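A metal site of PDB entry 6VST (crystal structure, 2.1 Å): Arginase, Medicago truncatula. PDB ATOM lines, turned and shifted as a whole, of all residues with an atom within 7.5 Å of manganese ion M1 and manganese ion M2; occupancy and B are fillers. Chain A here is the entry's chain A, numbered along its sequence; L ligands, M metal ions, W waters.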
ATOM      1  N   ASP A 159      -6.151 -23.309 -24.386  1.00  0.00           N
ATOM      2  CA  ASP A 159      -6.042 -21.860 -24.215  1.00  0.00           C
ATOM      3  C   ASP A 159      -4.666 -21.403 -24.686  1.00  0.00           C
ATOM      4  O   ASP A 159      -3.775 -22.206 -25.012  1.00  0.00           O
ATOM      5  CB  ASP A 159      -6.325 -21.426 -22.762  1.00  0.00           C
ATOM      6  CG  ASP A 159      -5.328 -21.981 -21.740  1.00  0.00           C
ATOM      7  OD1 ASP A 159      -4.090 -21.902 -21.976  1.00  0.00           O
ATOM      8  OD2 ASP A 159      -5.787 -22.453 -20.673  1.00  0.00           O
ATOM      9  N   HIS A 160      -4.478 -20.079 -24.720  1.00  0.00           N
ATOM     10  CA  HIS A 160      -3.301 -19.556 -25.399  1.00  0.00           C
ATOM     11  C   HIS A 160      -1.989 -19.806 -24.632  1.00  0.00           C
ATOM     12  O   HIS A 160      -0.922 -19.534 -25.177  1.00  0.00           O
ATOM     13  CB  HIS A 160      -3.476 -18.056 -25.670  1.00  0.00           C
ATOM     14  CG  HIS A 160      -2.877 -17.629 -26.972  1.00  0.00           C
ATOM     15  ND1 HIS A 160      -3.349 -16.559 -27.695  1.00  0.00           N
ATOM     16  CD2 HIS A 160      -1.869 -18.169 -27.711  1.00  0.00           C
ATOM     17  CE1 HIS A 160      -2.655 -16.439 -28.813  1.00  0.00           C
ATOM     18  NE2 HIS A 160      -1.749 -17.402 -28.847  1.00  0.00           N
ATOM     19  N   SER A 161      -2.044 -20.274 -23.382  1.00  0.00           N
ATOM     20  CA  SER A 161      -0.815 -20.579 -22.641  1.00  0.00           C
ATOM     21  C   SER A 161       0.054 -21.585 -23.371  1.00  0.00           C
ATOM     22  O   SER A 161       1.281 -21.585 -23.210  1.00  0.00           O
ATOM     23  CB  SER A 161      -1.142 -21.105 -21.252  1.00  0.00           C
ATOM     24  OG  SER A 161      -1.727 -22.405 -21.310  1.00  0.00           O
ATOM     25  N   SER A 163       1.010 -21.684 -26.362  1.00  0.00           N
ATOM     26  CA  SER A 163       1.949 -21.187 -27.363  1.00  0.00           C
ATOM     27  C   SER A 163       3.374 -21.092 -26.811  1.00  0.00           C
ATOM     28  O   SER A 163       4.347 -21.224 -27.561  1.00  0.00           O
ATOM     29  CB  SER A 163       1.474 -19.823 -27.871  1.00  0.00           C
ATOM     30  OG  SER A 163       0.377 -19.971 -28.744  1.00  0.00           O
ATOM     31  N   HIS A 182       1.034 -13.104 -34.998  1.00  0.00           N
ATOM     32  CA  HIS A 182       0.161 -13.397 -33.862  1.00  0.00           C
ATOM     33  C   HIS A 182      -1.150 -12.621 -34.036  1.00  0.00           C
ATOM     34  O   HIS A 182      -1.143 -11.378 -34.027  1.00  0.00           O
ATOM     35  CB  HIS A 182       0.880 -13.015 -32.566  1.00  0.00           C
ATOM     36  CG  HIS A 182       0.040 -13.094 -31.327  1.00  0.00           C
ATOM     37  ND1 HIS A 182       0.243 -12.267 -30.255  1.00  0.00           N
ATOM     38  CD2 HIS A 182      -0.973 -13.924 -30.975  1.00  0.00           C
ATOM     39  CE1 HIS A 182      -0.615 -12.570 -29.286  1.00  0.00           C
ATOM     40  NE2 HIS A 182      -1.339 -13.599 -29.697  1.00  0.00           N
ATOM     41  N   PHE A 183      -2.252 -13.349 -34.216  1.00  0.00           N
ATOM     42  CA  PHE A 183      -3.591 -12.766 -34.312  1.00  0.00           C
ATOM     43  C   PHE A 183      -4.287 -12.890 -32.969  1.00  0.00           C
ATOM     44  O   PHE A 183      -4.431 -14.001 -32.434  1.00  0.00           O
ATOM     45  CB  PHE A 183      -4.459 -13.481 -35.365  1.00  0.00           C
ATOM     46  CG  PHE A 183      -3.925 -13.381 -36.770  1.00  0.00           C
ATOM     47  CD1 PHE A 183      -4.246 -12.297 -37.572  1.00  0.00           C
ATOM     48  CD2 PHE A 183      -3.128 -14.385 -37.288  1.00  0.00           C
ATOM     49  CE1 PHE A 183      -3.770 -12.196 -38.867  1.00  0.00           C
ATOM     50  CE2 PHE A 183      -2.651 -14.296 -38.601  1.00  0.00           C
ATOM     51  CZ  PHE A 183      -2.974 -13.208 -39.390  1.00  0.00           C
ATOM     52  N   ASP A 184      -4.776 -11.766 -32.448  1.00  0.00           N
ATOM     53  CA  ASP A 184      -5.309 -11.796 -31.101  1.00  0.00           C
ATOM     54  C   ASP A 184      -6.032 -10.484 -30.809  1.00  0.00           C
ATOM     55  O   ASP A 184      -5.658  -9.426 -31.345  1.00  0.00           O
ATOM     56  CB  ASP A 184      -4.180 -12.029 -30.083  1.00  0.00           C
ATOM     57  CG  ASP A 184      -4.632 -12.810 -28.867  1.00  0.00           C
ATOM     58  OD1 ASP A 184      -5.741 -12.507 -28.377  1.00  0.00           O
ATOM     59  OD2 ASP A 184      -3.890 -13.739 -28.444  1.00  0.00           O
ATOM     60  N   ALA A 185      -7.090 -10.558 -29.987  1.00  0.00           N
ATOM     61  CA  ALA A 185      -7.639  -9.346 -29.382  1.00  0.00           C
ATOM     62  C   ALA A 185      -6.741  -8.799 -28.288  1.00  0.00           C
ATOM     63  O   ALA A 185      -6.850  -7.610 -27.945  1.00  0.00           O
ATOM     64  CB  ALA A 185      -9.022  -9.619 -28.803  1.00  0.00           C
ATOM     65  N   HIS A 186      -5.860  -9.641 -27.728  1.00  0.00           N
ATOM     66  CA  HIS A 186      -5.041  -9.382 -26.543  1.00  0.00           C
ATOM     67  C   HIS A 186      -3.564  -9.604 -26.835  1.00  0.00           C
ATOM     68  O   HIS A 186      -3.195 -10.617 -27.439  1.00  0.00           O
ATOM     69  CB  HIS A 186      -5.453 -10.286 -25.365  1.00  0.00           C
ATOM     70  CG  HIS A 186      -6.942 -10.403 -25.187  1.00  0.00           C
ATOM     71  ND1 HIS A 186      -7.701 -11.396 -25.771  1.00  0.00           N
ATOM     72  CD2 HIS A 186      -7.817  -9.631 -24.476  1.00  0.00           C
ATOM     73  CE1 HIS A 186      -8.967 -11.254 -25.429  1.00  0.00           C
ATOM     74  NE2 HIS A 186      -9.066 -10.185 -24.643  1.00  0.00           N
ATOM     75  N   PRO A 187      -2.688  -8.711 -26.367  1.00  0.00           N
ATOM     76  CA  PRO A 187      -1.248  -8.896 -26.594  1.00  0.00           C
ATOM     77  C   PRO A 187      -0.683 -10.121 -25.906  1.00  0.00           C
ATOM     78  O   PRO A 187       0.344 -10.618 -26.363  1.00  0.00           O
ATOM     79  CB  PRO A 187      -0.629  -7.608 -26.025  1.00  0.00           C
ATOM     80  CG  PRO A 187      -1.818  -6.625 -25.982  1.00  0.00           C
ATOM     81  CD  PRO A 187      -2.956  -7.487 -25.588  1.00  0.00           C
ATOM     82  N   ASP A 188      -1.332 -10.619 -24.829  1.00  0.00           N
ATOM     83  CA  ASP A 188      -0.865 -11.784 -24.062  1.00  0.00           C
ATOM     84  C   ASP A 188       0.584 -11.604 -23.600  1.00  0.00           C
ATOM     85  O   ASP A 188       1.400 -12.528 -23.660  1.00  0.00           O
ATOM     86  CB  ASP A 188      -1.013 -13.075 -24.871  1.00  0.00           C
ATOM     87  CG  ASP A 188      -2.475 -13.479 -25.087  1.00  0.00           C
ATOM     88  OD1 ASP A 188      -3.363 -12.913 -24.420  1.00  0.00           O
ATOM     89  OD2 ASP A 188      -2.713 -14.376 -25.911  1.00  0.00           O
ATOM     90  N   HIS A 200      -2.677 -17.928 -19.580  1.00  0.00           N
ATOM     91  CA  HIS A 200      -2.908 -17.733 -21.014  1.00  0.00           C
ATOM     92  C   HIS A 200      -2.782 -16.270 -21.429  1.00  0.00           C
ATOM     93  O   HIS A 200      -2.800 -15.978 -22.621  1.00  0.00           O
ATOM     94  CB  HIS A 200      -4.288 -18.285 -21.434  1.00  0.00           C
ATOM     95  CG  HIS A 200      -5.470 -17.477 -20.954  1.00  0.00           C
ATOM     96  ND1 HIS A 200      -6.657 -17.412 -21.653  1.00  0.00           N
ATOM     97  CD2 HIS A 200      -5.661 -16.730 -19.837  1.00  0.00           C
ATOM     98  CE1 HIS A 200      -7.520 -16.652 -21.004  1.00  0.00           C
ATOM     99  NE2 HIS A 200      -6.941 -16.239 -19.888  1.00  0.00           N
ATOM    100  N   ALA A 201      -2.689 -15.360 -20.474  1.00  0.00           N
ATOM    101  CA  ALA A 201      -2.472 -13.946 -20.748  1.00  0.00           C
ATOM    102  C   ALA A 201      -0.997 -13.583 -20.764  1.00  0.00           C
ATOM    103  O   ALA A 201      -0.668 -12.408 -20.931  1.00  0.00           O
ATOM    104  CB  ALA A 201      -3.216 -13.083 -19.723  1.00  0.00           C
ATOM    105  N   PRO A 203       1.745 -15.985 -22.418  1.00  0.00           N
ATOM    106  CA  PRO A 203       2.710 -16.814 -23.172  1.00  0.00           C
ATOM    107  C   PRO A 203       3.670 -16.004 -24.034  1.00  0.00           C
ATOM    108  O   PRO A 203       4.793 -16.473 -24.283  1.00  0.00           O
ATOM    109  CB  PRO A 203       1.809 -17.696 -24.052  1.00  0.00           C
ATOM    110  CG  PRO A 203       0.573 -16.776 -24.287  1.00  0.00           C
ATOM    111  CD  PRO A 203       0.372 -16.174 -22.941  1.00  0.00           C
ATOM    112  N   PHE A 204       3.285 -14.811 -24.490  1.00  0.00           N
ATOM    113  CA  PHE A 204       4.234 -14.089 -25.319  1.00  0.00           C
ATOM    114  C   PHE A 204       5.212 -13.274 -24.482  1.00  0.00           C
ATOM    115  O   PHE A 204       6.322 -12.985 -24.966  1.00  0.00           O
ATOM    116  CB  PHE A 204       3.501 -13.242 -26.359  1.00  0.00           C
ATOM    117  CG  PHE A 204       2.834 -14.107 -27.402  1.00  0.00           C
ATOM    118  CD1 PHE A 204       3.571 -14.583 -28.487  1.00  0.00           C
ATOM    119  CD2 PHE A 204       1.537 -14.561 -27.210  1.00  0.00           C
ATOM    120  CE1 PHE A 204       2.984 -15.444 -29.413  1.00  0.00           C
ATOM    121  CE2 PHE A 204       0.945 -15.435 -28.134  1.00  0.00           C
ATOM    122  CZ  PHE A 204       1.676 -15.867 -29.233  1.00  0.00           C
ATOM    123  N   ILE A 221      -5.423  -6.267 -32.151  1.00  0.00           N
ATOM    124  CA  ILE A 221      -5.376  -5.908 -30.743  1.00  0.00           C
ATOM    125  C   ILE A 221      -6.366  -4.788 -30.441  1.00  0.00           C
ATOM    126  O   ILE A 221      -6.391  -3.744 -31.102  1.00  0.00           O
ATOM    127  CB  ILE A 221      -3.947  -5.498 -30.332  1.00  0.00           C
ATOM    128  CG1 ILE A 221      -2.946  -6.657 -30.590  1.00  0.00           C
ATOM    129  CG2 ILE A 221      -3.944  -5.029 -28.882  1.00  0.00           C
ATOM    130  CD1 ILE A 221      -3.131  -7.841 -29.702  1.00  0.00           C
ATOM    131  N   SER A 267       0.548 -17.843 -34.763  1.00  0.00           N
ATOM    132  CA  SER A 267      -0.373 -18.145 -33.662  1.00  0.00           C
ATOM    133  C   SER A 267      -1.692 -17.421 -33.903  1.00  0.00           C
ATOM    134  O   SER A 267      -1.724 -16.188 -34.010  1.00  0.00           O
ATOM    135  CB  SER A 267       0.216 -17.758 -32.305  1.00  0.00           C
ATOM    136  OG  SER A 267      -0.668 -18.050 -31.210  1.00  0.00           O
ATOM    137  N   ILE A 268      -2.780 -18.179 -33.997  1.00  0.00           N
ATOM    138  CA  ILE A 268      -4.096 -17.630 -34.318  1.00  0.00           C
ATOM    139  C   ILE A 268      -4.996 -17.844 -33.114  1.00  0.00           C
ATOM    140  O   ILE A 268      -5.432 -18.971 -32.844  1.00  0.00           O
ATOM    141  CB  ILE A 268      -4.711 -18.259 -35.575  1.00  0.00           C
ATOM    142  CG1 ILE A 268      -3.672 -18.352 -36.686  1.00  0.00           C
ATOM    143  CG2 ILE A 268      -5.958 -17.441 -36.013  1.00  0.00           C
ATOM    144  CD1 ILE A 268      -4.231 -18.817 -38.036  1.00  0.00           C
ATOM    145  N   ASP A 269      -5.291 -16.762 -32.386  1.00  0.00           N
ATOM    146  CA  ASP A 269      -6.263 -16.808 -31.312  1.00  0.00           C
ATOM    147  C   ASP A 269      -7.634 -16.511 -31.909  1.00  0.00           C
ATOM    148  O   ASP A 269      -7.826 -15.443 -32.513  1.00  0.00           O
ATOM    149  CB  ASP A 269      -5.882 -15.811 -30.212  1.00  0.00           C
ATOM    150  CG  ASP A 269      -6.822 -15.857 -29.006  1.00  0.00           C
ATOM    151  OD1 ASP A 269      -8.028 -16.188 -29.145  1.00  0.00           O
ATOM    152  OD2 ASP A 269      -6.326 -15.566 -27.904  1.00  0.00           O
ATOM    153  N   VAL A 270      -8.581 -17.439 -31.764  1.00  0.00           N
ATOM    154  CA  VAL A 270      -9.893 -17.260 -32.390  1.00  0.00           C
ATOM    155  C   VAL A 270     -10.581 -15.998 -31.860  1.00  0.00           C
ATOM    156  O   VAL A 270     -11.387 -15.405 -32.572  1.00  0.00           O
ATOM    157  CB  VAL A 270     -10.761 -18.539 -32.222  1.00  0.00           C
ATOM    158  CG1 VAL A 270     -12.176 -18.343 -32.795  1.00  0.00           C
ATOM    159  CG2 VAL A 270     -10.106 -19.740 -32.948  1.00  0.00           C
ATOM    160  N   ASP A 271     -10.244 -15.507 -30.664  1.00  0.00           N
ATOM    161  CA  ASP A 271     -10.928 -14.296 -30.208  1.00  0.00           C
ATOM    162  C   ASP A 271     -10.408 -13.023 -30.884  1.00  0.00           C
ATOM    163  O   ASP A 271     -10.887 -11.923 -30.564  1.00  0.00           O
ATOM    164  CB  ASP A 271     -10.881 -14.191 -28.685  1.00  0.00           C
ATOM    165  CG  ASP A 271      -9.521 -13.780 -28.120  1.00  0.00           C
ATOM    166  OD1 ASP A 271      -8.665 -13.211 -28.827  1.00  0.00           O
ATOM    167  OD2 ASP A 271      -9.340 -14.037 -26.906  1.00  0.00           O
ATOM    168  N   SER A 272      -9.451 -13.133 -31.808  1.00  0.00           N
ATOM    169  CA  SER A 272      -9.119 -11.994 -32.652  1.00  0.00           C
ATOM    170  C   SER A 272     -10.291 -11.617 -33.548  1.00  0.00           C
ATOM    171  O   SER A 272     -10.464 -10.441 -33.884  1.00  0.00           O
ATOM    172  CB  SER A 272      -7.883 -12.289 -33.483  1.00  0.00           C
ATOM    173  OG  SER A 272      -8.092 -13.393 -34.358  1.00  0.00           O
ATOM    174  N   HIS A 283     -13.202 -14.911 -24.167  1.00  0.00           N
ATOM    175  CA  HIS A 283     -13.066 -13.463 -24.022  1.00  0.00           C
ATOM    176  C   HIS A 283     -13.667 -12.739 -25.220  1.00  0.00           C
ATOM    177  O   HIS A 283     -12.993 -12.475 -26.220  1.00  0.00           O
ATOM    178  CB  HIS A 283     -11.617 -13.098 -23.795  1.00  0.00           C
ATOM    179  CG  HIS A 283     -11.076 -13.718 -22.541  1.00  0.00           C
ATOM    180  ND1 HIS A 283     -11.233 -13.128 -21.303  1.00  0.00           N
ATOM    181  CD2 HIS A 283     -10.486 -14.908 -22.315  1.00  0.00           C
ATOM    182  CE1 HIS A 283     -10.722 -13.914 -20.377  1.00  0.00           C
ATOM    183  NE2 HIS A 283     -10.271 -15.004 -20.966  1.00  0.00           N
ATOM    184  N   VAL A 311      -5.889 -21.401 -31.302  1.00  0.00           N
ATOM    185  CA  VAL A 311      -6.179 -21.523 -29.874  1.00  0.00           C
ATOM    186  C   VAL A 311      -7.452 -20.762 -29.513  1.00  0.00           C
ATOM    187  O   VAL A 311      -7.922 -19.895 -30.249  1.00  0.00           O
ATOM    188  CB  VAL A 311      -4.994 -21.042 -28.991  1.00  0.00           C
ATOM    189  CG1 VAL A 311      -3.711 -21.814 -29.317  1.00  0.00           C
ATOM    190  CG2 VAL A 311      -4.770 -19.528 -29.137  1.00  0.00           C
ATOM    191  N   GLU A 312      -7.988 -21.111 -28.338  1.00  0.00           N
ATOM    192  CA  GLU A 312      -9.042 -20.425 -27.599  1.00  0.00           C
ATOM    193  C   GLU A 312     -10.428 -20.643 -28.189  1.00  0.00           C
ATOM    194  O   GLU A 312     -11.360 -19.993 -27.734  1.00  0.00           O
ATOM    195  CB  GLU A 312      -8.797 -18.918 -27.440  1.00  0.00           C
ATOM    196  CG  GLU A 312      -7.548 -18.543 -26.590  1.00  0.00           C
ATOM    197  CD  GLU A 312      -7.773 -18.540 -25.070  1.00  0.00           C
ATOM    198  OE1 GLU A 312      -8.924 -18.467 -24.577  1.00  0.00           O
ATOM    199  OE2 GLU A 312      -6.756 -18.578 -24.339  1.00  0.00           O
HETATM  200  N1  LIG L   1      -8.500 -10.341 -19.369  1.00  0.00           N
HETATM  201  C1  LIG L   1      -7.285 -10.752 -20.115  1.00  0.00           C
HETATM  202  C2  LIG L   1      -7.675 -11.702 -21.253  1.00  0.00           C
HETATM  203  C3  LIG L   1      -6.578 -12.656 -21.724  1.00  0.00           C
HETATM  204  C4  LIG L   1      -7.072 -13.642 -22.778  1.00  0.00           C
HETATM  205  N2  LIG L   1      -6.073 -14.512 -23.409  1.00  0.00           N
HETATM  206  C5  LIG L   1      -6.556  -9.487 -20.607  1.00  0.00           C
HETATM  207  O1  LIG L   1      -6.501  -8.505 -19.808  1.00  0.00           O
HETATM  208  O2  LIG L   1      -6.053  -9.511 -21.755  1.00  0.00           O
HETATM  209 MN    MN M   1      -7.101 -13.403 -26.961  1.00  0.00          MN
HETATM  210 MN    MN M   2      -4.374 -14.930 -26.979  1.00  0.00          MN
HETATM  211  O   HOH W   1      -5.421 -14.382 -25.628  1.00  0.00           O
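OD1 of Asp 188 lies within salt-bridge range of N2 of the ligand, at 3.3 Å.
ND1 of His 200 lies within hydrogen-bond range of N2 of the ligand, 3.4 Å away.
NE2 of His 182 sits close to OD2 of Asp 184 (2.8 Å).
O of Asp 184 is in hydrogen-bond range of N of Ile 221, at 3.3 Å.
O of Asp 188 lies within hydrogen-bond range of N of Phe 204 (3.1 Å).
The backbone NH of His 160 is in hydrogen-bond range of the side-chain carboxylate of Glu 312 (2.8 Å).
OG of Ser 267 lies within hydrogen-bond range of NE2 of His 160 (2.7 Å).
A ring nitrogen (NE2) of His 160 lies close to the side-chain hydroxyl of Ser 163 (3.3 Å).
O of Asp 269 is in hydrogen-bond range of OG of Ser 272, 2.8 Å away.
The side-chain carboxylate (OD1) of Asp 271 sits close to the backbone NH (N) of Ala 185, at 3.3 Å.
Four residues have an atom within 4 Å of manganese ion M1: Asp 184, His 186, Asp 269 and Asp 271.
The nearest printed residue that does not touch manganese ion M1 is Ala 185 (4.2 Å).
Four residues have an atom within 4 Å of manganese ion M2: His 160, Asp 184, Asp 188 and Asp 269.
Manganese ion M1 is bound by OD1 of Asp 184 (2.2 Å), OD2 of Asp 271 (2.3 Å), water W1 (2.4 Å), ND1 of His 186 (2.4 Å), OD1 of Asp 271 (2.4 Å) and OD2 of Asp 269 (2.5 Å).
Manganese ion M2 is bound by water W1 (1.8 Å).
OD2 of Asp 184 is bound to manganese ion M2, 1.9 Å away.
Manganese ion M2 is bound by OD2 of Asp 188, 2.1 Å away.
ND1 of His 160 is bound to manganese ion M2 (2.1 Å).
Manganese ion M2 is bound by OD2 of Asp 269 (2.3 Å).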
